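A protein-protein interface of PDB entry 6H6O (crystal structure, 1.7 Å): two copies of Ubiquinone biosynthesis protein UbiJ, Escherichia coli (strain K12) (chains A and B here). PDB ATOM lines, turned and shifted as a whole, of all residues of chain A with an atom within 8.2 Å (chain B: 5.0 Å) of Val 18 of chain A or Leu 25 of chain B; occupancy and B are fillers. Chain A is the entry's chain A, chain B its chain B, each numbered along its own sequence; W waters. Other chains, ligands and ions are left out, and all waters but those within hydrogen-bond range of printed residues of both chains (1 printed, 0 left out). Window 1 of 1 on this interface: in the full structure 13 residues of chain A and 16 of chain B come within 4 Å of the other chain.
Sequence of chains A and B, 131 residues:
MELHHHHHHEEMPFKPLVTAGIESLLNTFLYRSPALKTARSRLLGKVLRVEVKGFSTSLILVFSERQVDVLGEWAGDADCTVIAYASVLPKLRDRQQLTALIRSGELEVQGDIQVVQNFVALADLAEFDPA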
ATOM      1  N   MET A  12     -19.124   6.799  28.173  1.00  0.00           N
ATOM      2  CA  MET A  12     -20.032   7.291  27.129  1.00  0.00           C
ATOM      3  C   MET A  12     -20.745   8.565  27.618  1.00  0.00           C
ATOM      4  O   MET A  12     -21.405   8.489  28.659  1.00  0.00           O
ATOM      5  CB  MET A  12     -21.082   6.217  26.773  1.00  0.00           C
ATOM      6  CG  MET A  12     -20.520   5.019  26.027  1.00  0.00           C
ATOM      7  SD  MET A  12     -20.278   5.337  24.262  1.00  0.00           S
ATOM      8  CE  MET A  12     -21.978   5.295  23.676  1.00  0.00           C
ATOM      9  N   PRO A  13     -20.653   9.729  26.913  1.00  0.00           N
ATOM     10  CA  PRO A  13     -21.369  10.939  27.381  1.00  0.00           C
ATOM     11  C   PRO A  13     -22.870  10.703  27.537  1.00  0.00           C
ATOM     12  O   PRO A  13     -23.451   9.925  26.775  1.00  0.00           O
ATOM     13  CB  PRO A  13     -21.058  11.986  26.307  1.00  0.00           C
ATOM     14  CG  PRO A  13     -20.684  11.172  25.089  1.00  0.00           C
ATOM     15  CD  PRO A  13     -19.937   9.998  25.648  1.00  0.00           C
ATOM     16  N   PHE A  14     -23.490  11.375  28.519  1.00  0.00           N
ATOM     17  CA  PHE A  14     -24.899  11.157  28.868  1.00  0.00           C
ATOM     18  C   PHE A  14     -25.899  11.597  27.809  1.00  0.00           C
ATOM     19  O   PHE A  14     -26.808  10.814  27.485  1.00  0.00           O
ATOM     20  CB  PHE A  14     -25.232  11.809  30.220  1.00  0.00           C
ATOM     21  CG  PHE A  14     -26.528  11.357  30.848  1.00  0.00           C
ATOM     22  CD1 PHE A  14     -26.708  10.031  31.240  1.00  0.00           C
ATOM     23  CD2 PHE A  14     -27.577  12.252  31.037  1.00  0.00           C
ATOM     24  CE1 PHE A  14     -27.903   9.617  31.837  1.00  0.00           C
ATOM     25  CE2 PHE A  14     -28.779  11.830  31.620  1.00  0.00           C
ATOM     26  CZ  PHE A  14     -28.933  10.517  32.011  1.00  0.00           C
ATOM     27  N   LYS A  15     -25.797  12.861  27.340  1.00  0.00           N
ATOM     28  CA  LYS A  15     -26.744  13.420  26.373  1.00  0.00           C
ATOM     29  C   LYS A  15     -26.919  12.546  25.109  1.00  0.00           C
ATOM     30  O   LYS A  15     -28.067  12.232  24.830  1.00  0.00           O
ATOM     31  CB  LYS A  15     -26.394  14.891  26.018  1.00  0.00           C
ATOM     32  CG  LYS A  15     -27.308  15.538  24.971  1.00  0.00           C
ATOM     33  CD  LYS A  15     -28.547  16.189  25.575  1.00  0.00           C
ATOM     34  CE  LYS A  15     -29.616  16.424  24.529  1.00  0.00           C
ATOM     35  NZ  LYS A  15     -29.318  17.606  23.678  1.00  0.00           N
ATOM     36  N   PRO A  16     -25.859  12.108  24.360  1.00  0.00           N
ATOM     37  CA  PRO A  16     -26.092  11.243  23.179  1.00  0.00           C
ATOM     38  C   PRO A  16     -26.785   9.913  23.513  1.00  0.00           C
ATOM     39  O   PRO A  16     -27.543   9.408  22.686  1.00  0.00           O
ATOM     40  CB  PRO A  16     -24.682  11.033  22.599  1.00  0.00           C
ATOM     41  CG  PRO A  16     -23.860  12.124  23.175  1.00  0.00           C
ATOM     42  CD  PRO A  16     -24.409  12.354  24.541  1.00  0.00           C
ATOM     43  N   LEU A  17     -26.568   9.374  24.740  1.00  0.00           N
ATOM     44  CA  LEU A  17     -27.256   8.148  25.175  1.00  0.00           C
ATOM     45  C   LEU A  17     -28.749   8.413  25.357  1.00  0.00           C
ATOM     46  O   LEU A  17     -29.564   7.563  25.009  1.00  0.00           O
ATOM     47  CB  LEU A  17     -26.653   7.602  26.481  1.00  0.00           C
ATOM     48  CG  LEU A  17     -25.298   6.918  26.370  1.00  0.00           C
ATOM     49  CD1 LEU A  17     -24.847   6.472  27.755  1.00  0.00           C
ATOM     50  CD2 LEU A  17     -25.342   5.717  25.388  1.00  0.00           C
ATOM     51  N   VAL A  18     -29.108   9.599  25.898  1.00  0.00           N
ATOM     52  CA  VAL A  18     -30.513   9.998  26.087  1.00  0.00           C
ATOM     53  C   VAL A  18     -31.208  10.174  24.705  1.00  0.00           C
ATOM     54  O   VAL A  18     -32.312   9.643  24.492  1.00  0.00           O
ATOM     55  CB  VAL A  18     -30.631  11.260  26.983  1.00  0.00           C
ATOM     56  CG1 VAL A  18     -32.036  11.864  26.942  1.00  0.00           C
ATOM     57  CG2 VAL A  18     -30.192  10.954  28.424  1.00  0.00           C
ATOM     58  N   THR A  19     -30.570  10.926  23.770  1.00  0.00           N
ATOM     59  CA  THR A  19     -31.180  11.136  22.439  1.00  0.00           C
ATOM     60  C   THR A  19     -31.350   9.803  21.680  1.00  0.00           C
ATOM     61  O   THR A  19     -32.414   9.569  21.095  1.00  0.00           O
ATOM     62  CB  THR A  19     -30.448  12.206  21.644  1.00  0.00           C
ATOM     63  OG1 THR A  19     -29.124  11.767  21.411  1.00  0.00           O
ATOM     64  CG2 THR A  19     -30.426  13.538  22.356  1.00  0.00           C
ATOM     65  N   ALA A  20     -30.339   8.921  21.737  1.00  0.00           N
ATOM     66  CA  ALA A  20     -30.410   7.583  21.109  1.00  0.00           C
ATOM     67  C   ALA A  20     -31.561   6.726  21.686  1.00  0.00           C
ATOM     68  O   ALA A  20     -32.273   6.068  20.920  1.00  0.00           O
ATOM     69  CB  ALA A  20     -29.082   6.856  21.255  1.00  0.00           C
ATOM     70  N   GLY A  21     -31.746   6.780  23.012  1.00  0.00           N
ATOM     71  CA  GLY A  21     -32.810   6.068  23.729  1.00  0.00           C
ATOM     72  C   GLY A  21     -34.188   6.568  23.325  1.00  0.00           C
ATOM     73  O   GLY A  21     -35.088   5.770  23.024  1.00  0.00           O
ATOM     74  N   ILE A  22     -34.349   7.893  23.251  1.00  0.00           N
ATOM     75  CA  ILE A  22     -35.621   8.490  22.818  1.00  0.00           C
ATOM     76  C   ILE A  22     -35.917   8.078  21.377  1.00  0.00           C
ATOM     77  O   ILE A  22     -37.050   7.712  21.078  1.00  0.00           O
ATOM     78  CB  ILE A  22     -35.658  10.043  23.054  1.00  0.00           C
ATOM     79  CG1 ILE A  22     -35.663  10.349  24.569  1.00  0.00           C
ATOM     80  CG2 ILE A  22     -36.886  10.709  22.381  1.00  0.00           C
ATOM     81  CD1 ILE A  22     -35.304  11.837  24.881  1.00  0.00           C
ATOM     82  N   GLU A  23     -34.895   8.108  20.493  1.00  0.00           N
ATOM     83  CA  GLU A  23     -35.057   7.724  19.088  1.00  0.00           C
ATOM     84  C   GLU A  23     -35.536   6.265  18.983  1.00  0.00           C
ATOM     85  O   GLU A  23     -36.490   5.982  18.243  1.00  0.00           O
ATOM     86  CB  GLU A  23     -33.735   7.914  18.316  1.00  0.00           C
ATOM     87  CG  GLU A  23     -33.858   7.534  16.851  1.00  0.00           C
ATOM     88  CD  GLU A  23     -32.659   7.890  15.992  1.00  0.00           C
ATOM     89  OE1 GLU A  23     -32.200   9.053  16.067  1.00  0.00           O
ATOM     90  OE2 GLU A  23     -32.239   7.036  15.178  1.00  0.00           O
ATOM     91  N   SER A  24     -34.881   5.345  19.739  1.00  0.00           N
ATOM     92  CA  SER A  24     -35.259   3.934  19.734  1.00  0.00           C
ATOM     93  C   SER A  24     -36.731   3.752  20.173  1.00  0.00           C
ATOM     94  O   SER A  24     -37.485   3.042  19.510  1.00  0.00           O
ATOM     95  CB  SER A  24     -34.324   3.135  20.642  1.00  0.00           C
ATOM     96  OG  SER A  24     -34.689   1.768  20.628  1.00  0.00           O
ATOM     97  N   LEU A  25     -37.125   4.427  21.261  1.00  0.00           N
ATOM     98  CA  LEU A  25     -38.484   4.391  21.823  1.00  0.00           C
ATOM     99  C   LEU A  25     -39.499   4.879  20.783  1.00  0.00           C
ATOM    100  O   LEU A  25     -40.486   4.185  20.541  1.00  0.00           O
ATOM    101  CB  LEU A  25     -38.582   5.273  23.075  1.00  0.00           C
ATOM    102  CG  LEU A  25     -38.408   4.596  24.462  1.00  0.00           C
ATOM    103  CD1 LEU A  25     -38.198   5.627  25.531  1.00  0.00           C
ATOM    104  CD2 LEU A  25     -39.648   3.804  24.828  1.00  0.00           C
ATOM    105  N   PHE A  55     -34.527  21.869  31.413  1.00  0.00           N
ATOM    106  CA  PHE A  55     -33.406  21.159  30.792  1.00  0.00           C
ATOM    107  C   PHE A  55     -32.628  22.170  29.946  1.00  0.00           C
ATOM    108  O   PHE A  55     -33.229  23.056  29.336  1.00  0.00           O
ATOM    109  CB  PHE A  55     -33.902  19.977  29.945  1.00  0.00           C
ATOM    110  CG  PHE A  55     -34.454  18.841  30.765  1.00  0.00           C
ATOM    111  CD1 PHE A  55     -35.761  18.877  31.244  1.00  0.00           C
ATOM    112  CD2 PHE A  55     -33.668  17.738  31.068  1.00  0.00           C
ATOM    113  CE1 PHE A  55     -36.270  17.824  32.008  1.00  0.00           C
ATOM    114  CE2 PHE A  55     -34.187  16.673  31.805  1.00  0.00           C
ATOM    115  CZ  PHE A  55     -35.486  16.720  32.263  1.00  0.00           C
ATOM    116  N   THR A  57     -30.812  21.583  27.227  1.00  0.00           N
ATOM    117  CA  THR A  57     -30.695  21.205  25.819  1.00  0.00           C
ATOM    118  C   THR A  57     -32.037  20.974  25.115  1.00  0.00           C
ATOM    119  O   THR A  57     -33.019  20.614  25.742  1.00  0.00           O
ATOM    120  CB  THR A  57     -29.824  19.947  25.699  1.00  0.00           C
ATOM    121  OG1 THR A  57     -30.344  18.936  26.568  1.00  0.00           O
ATOM    122  CG2 THR A  57     -28.338  20.213  25.968  1.00  0.00           C
ATOM    123  N   SER A  58     -32.038  21.108  23.797  1.00  0.00           N
ATOM    124  CA  SER A  58     -33.198  20.887  22.928  1.00  0.00           C
ATOM    125  C   SER A  58     -33.240  19.413  22.453  1.00  0.00           C
ATOM    126  O   SER A  58     -32.225  18.710  22.509  1.00  0.00           O
ATOM    127  CB  SER A  58     -33.087  21.794  21.700  1.00  0.00           C
ATOM    128  OG  SER A  58     -32.827  23.145  22.040  1.00  0.00           O
ATOM    129  N   LEU A  59     -34.415  18.975  21.975  1.00  0.00           N
ATOM    130  CA  LEU A  59     -34.621  17.687  21.319  1.00  0.00           C
ATOM    131  C   LEU A  59     -35.172  18.044  19.928  1.00  0.00           C
ATOM    132  O   LEU A  59     -36.092  18.844  19.818  1.00  0.00           O
ATOM    133  CB  LEU A  59     -35.653  16.811  22.034  1.00  0.00           C
ATOM    134  CG  LEU A  59     -35.239  16.103  23.332  1.00  0.00           C
ATOM    135  CD1 LEU A  59     -36.424  15.340  23.882  1.00  0.00           C
ATOM    136  CD2 LEU A  59     -34.072  15.100  23.102  1.00  0.00           C
ATOM    137  N   VAL A  70     -33.680  11.493  16.092  1.00  0.00           N
ATOM    138  CA  VAL A  70     -33.663  12.412  17.209  1.00  0.00           C
ATOM    139  C   VAL A  70     -32.235  12.966  17.331  1.00  0.00           C
ATOM    140  O   VAL A  70     -31.275  12.188  17.333  1.00  0.00           O
ATOM    141  CB  VAL A  70     -34.190  11.810  18.540  1.00  0.00           C
ATOM    142  CG1 VAL A  70     -34.209  12.861  19.644  1.00  0.00           C
ATOM    143  CG2 VAL A  70     -35.594  11.227  18.354  1.00  0.00           C
ATOM    144  N   GLY B  21     -35.817   1.017  27.706  1.00  0.00           N
ATOM    145  CA  GLY B  21     -34.988   2.131  27.244  1.00  0.00           C
ATOM    146  C   GLY B  21     -34.170   2.734  28.368  1.00  0.00           C
ATOM    147  O   GLY B  21     -32.958   2.934  28.230  1.00  0.00           O
ATOM    148  N   ILE B  22     -34.819   2.967  29.531  1.00  0.00           N
ATOM    149  CA  ILE B  22     -34.125   3.482  30.712  1.00  0.00           C
ATOM    150  C   ILE B  22     -33.066   2.479  31.193  1.00  0.00           C
ATOM    151  O   ILE B  22     -31.942   2.881  31.502  1.00  0.00           O
ATOM    152  CB  ILE B  22     -35.111   3.922  31.820  1.00  0.00           C
ATOM    153  CG1 ILE B  22     -35.933   5.161  31.309  1.00  0.00           C
ATOM    154  CG2 ILE B  22     -34.319   4.253  33.142  1.00  0.00           C
ATOM    155  CD1 ILE B  22     -37.159   5.494  32.087  1.00  0.00           C
ATOM    156  N   GLU B  23     -33.402   1.180  31.189  1.00  0.00           N
ATOM    157  CA  GLU B  23     -32.450   0.137  31.603  1.00  0.00           C
ATOM    158  C   GLU B  23     -31.215   0.149  30.696  1.00  0.00           C
ATOM    159  O   GLU B  23     -30.094   0.123  31.202  1.00  0.00           O
ATOM    160  CB  GLU B  23     -33.115  -1.244  31.594  1.00  0.00           C
ATOM    161  CG  GLU B  23     -32.173  -2.339  32.056  1.00  0.00           C
ATOM    162  CD  GLU B  23     -32.878  -3.661  32.279  1.00  0.00           C
ATOM    163  OE1 GLU B  23     -33.926  -3.680  32.971  1.00  0.00           O
ATOM    164  OE2 GLU B  23     -32.326  -4.691  31.832  1.00  0.00           O
ATOM    165  N   SER B  24     -31.427   0.207  29.370  1.00  0.00           N
ATOM    166  CA  SER B  24     -30.326   0.234  28.390  1.00  0.00           C
ATOM    167  C   SER B  24     -29.432   1.471  28.611  1.00  0.00           C
ATOM    168  O   SER B  24     -28.213   1.342  28.663  1.00  0.00           O
ATOM    169  CB  SER B  24     -30.883   0.213  26.972  1.00  0.00           C
ATOM    170  OG  SER B  24     -29.834   0.244  26.020  1.00  0.00           O
ATOM    171  N   LEU B  25     -30.040   2.644  28.799  1.00  0.00           N
ATOM    172  CA  LEU B  25     -29.332   3.895  29.070  1.00  0.00           C
ATOM    173  C   LEU B  25     -28.468   3.780  30.334  1.00  0.00           C
ATOM    174  O   LEU B  25     -27.281   4.096  30.275  1.00  0.00           O
ATOM    175  CB  LEU B  25     -30.357   5.044  29.226  1.00  0.00           C
ATOM    176  CG  LEU B  25     -29.834   6.341  29.833  1.00  0.00           C
ATOM    177  CD1 LEU B  25     -29.048   7.120  28.821  1.00  0.00           C
ATOM    178  CD2 LEU B  25     -30.975   7.211  30.311  1.00  0.00           C
ATOM    179  N   LEU B  26     -29.053   3.301  31.453  1.00  0.00           N
ATOM    180  CA  LEU B  26     -28.314   3.185  32.710  1.00  0.00           C
ATOM    181  C   LEU B  26     -27.184   2.184  32.640  1.00  0.00           C
ATOM    182  O   LEU B  26     -26.112   2.452  33.187  1.00  0.00           O
ATOM    183  CB  LEU B  26     -29.236   2.918  33.907  1.00  0.00           C
ATOM    184  CG  LEU B  26     -30.261   4.016  34.245  1.00  0.00           C
ATOM    185  CD1 LEU B  26     -31.225   3.524  35.314  1.00  0.00           C
ATOM    186  CD2 LEU B  26     -29.563   5.309  34.725  1.00  0.00           C
ATOM    187  N   ASN B  27     -27.402   1.040  31.966  1.00  0.00           N
ATOM    188  CA  ASN B  27     -26.355   0.034  31.854  1.00  0.00           C
ATOM    189  C   ASN B  27     -25.196   0.495  30.965  1.00  0.00           C
ATOM    190  O   ASN B  27     -24.031   0.321  31.334  1.00  0.00           O
ATOM    191  CB  ASN B  27     -26.944  -1.295  31.412  1.00  0.00           C
ATOM    192  CG  ASN B  27     -27.571  -1.993  32.585  1.00  0.00           C
ATOM    193  OD1 ASN B  27     -26.994  -2.037  33.683  1.00  0.00           O
ATOM    194  ND2 ASN B  27     -28.778  -2.486  32.406  1.00  0.00           N
ATOM    195  N   THR B  28     -25.501   1.176  29.853  1.00  0.00           N
ATOM    196  CA  THR B  28     -24.410   1.703  29.018  1.00  0.00           C
ATOM    197  C   THR B  28     -23.634   2.788  29.779  1.00  0.00           C
ATOM    198  O   THR B  28     -22.403   2.854  29.677  1.00  0.00           O
ATOM    199  CB  THR B  28     -24.941   2.243  27.677  1.00  0.00           C
ATOM    200  OG1 THR B  28     -25.713   1.227  27.042  1.00  0.00           O
ATOM    201  CG2 THR B  28     -23.811   2.729  26.742  1.00  0.00           C
ATOM    202  N   PHE B  29     -24.341   3.608  30.559  1.00  0.00           N
ATOM    203  CA  PHE B  29     -23.724   4.715  31.286  1.00  0.00           C
ATOM    204  C   PHE B  29     -22.908   4.269  32.532  1.00  0.00           C
ATOM    205  O   PHE B  29     -21.779   4.737  32.723  1.00  0.00           O
ATOM    206  CB  PHE B  29     -24.784   5.770  31.647  1.00  0.00           C
ATOM    207  CG  PHE B  29     -24.269   7.034  32.311  1.00  0.00           C
ATOM    208  CD1 PHE B  29     -23.406   7.891  31.640  1.00  0.00           C
ATOM    209  CD2 PHE B  29     -24.673   7.379  33.599  1.00  0.00           C
ATOM    210  CE1 PHE B  29     -22.951   9.073  32.245  1.00  0.00           C
ATOM    211  CE2 PHE B  29     -24.185   8.542  34.218  1.00  0.00           C
ATOM    212  CZ  PHE B  29     -23.343   9.383  33.532  1.00  0.00           C
ATOM    213  N   LEU B  30     -23.462   3.336  33.320  1.00  0.00           N
ATOM    214  CA  LEU B  30     -22.888   2.924  34.608  1.00  0.00           C
ATOM    215  C   LEU B  30     -22.167   1.591  34.655  1.00  0.00           C
ATOM    216  O   LEU B  30     -21.238   1.436  35.465  1.00  0.00           O
ATOM    217  CB  LEU B  30     -24.009   2.915  35.682  1.00  0.00           C
ATOM    218  CG  LEU B  30     -24.797   4.203  35.882  1.00  0.00           C
ATOM    219  CD1 LEU B  30     -25.979   3.951  36.786  1.00  0.00           C
ATOM    220  CD2 LEU B  30     -23.887   5.353  36.410  1.00  0.00           C
HETATM  221  O   HOH W   1     -19.847   6.214  31.535  1.00  0.00           O
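Positions printed for both chains: 21, 22, 23, 24 and 25.
Of the 6 pairs that touch across the chains among the printed residues, none has its exchanged pair printed and touching as well.
Among the printed residues, pairs that only touch across the chains: Leu 17 of chain A with Leu 25 of chain B, Leu 17 of chain A with Thr 28 of chain B, Met 12 of chain A with Phe 29 of chain B, Val 18 of chain A with Leu 25 of chain B, Phe 14 of chain A with Phe 29 of chain B and Leu 17 of chain A with Phe 29 of chain B.
Printed residues of chain B within 4 Å of Met 12 of chain A: Phe 29.
Of the printed residues of chain B, Phe 14 of chain A touches Phe 29 (3.96 Å).
Of chain B, only Leu 25 (3.8 Å) comes within 4 Å of Val 18 of chain A.
Ile 22 of chain A touches none of the printed residues of chain B.
Gly 21 of chain B touches none of the printed residues of chain A.
No residue of chain A comes within 4 Å of Ser 24 of chain B.
Leu 25 of chain B touches just these residues of chain A: Leu 17 and Val 18.
Of the printed residues of chain A, Phe 29 of chain B touches Met 12 (3.6 Å), Phe 14 (3.96 Å) and Leu 17 (3.96 Å).
The nearest printed residue of chain A that does not touch Thr 28 of chain B is Met 12 of chain A (4.1 Å).
OG1 of Thr 28 of chain B is in hydrogen-bond range of O of Ser 24 of chain B (3.0 Å).
Water W1 lies within hydrogen-bond range of O of Phe 29 of chain B and N of Met 12 of chain A.
Of the 10 printed residues of chain B, 3 touch a printed residue of chain A.
Hydrophobic or aromatic side chains of chain B within 4 Å of the printed part of chain A: Leu 25 and Phe 29.
Along chain B the printed residues that touch a printed residue of chain A span positions 25 to 29.
Of the 19 printed residues of chain A, 4 touch a printed residue of chain B.
Hydrophobic or aromatic side chains of chain A that line the printed part of chain B: Phe 14 and Leu 17.
Among the printed residues, no Asp or Glu carboxylate lies within 4 Å of a Lys or Arg side-chain nitrogen of the other chain.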
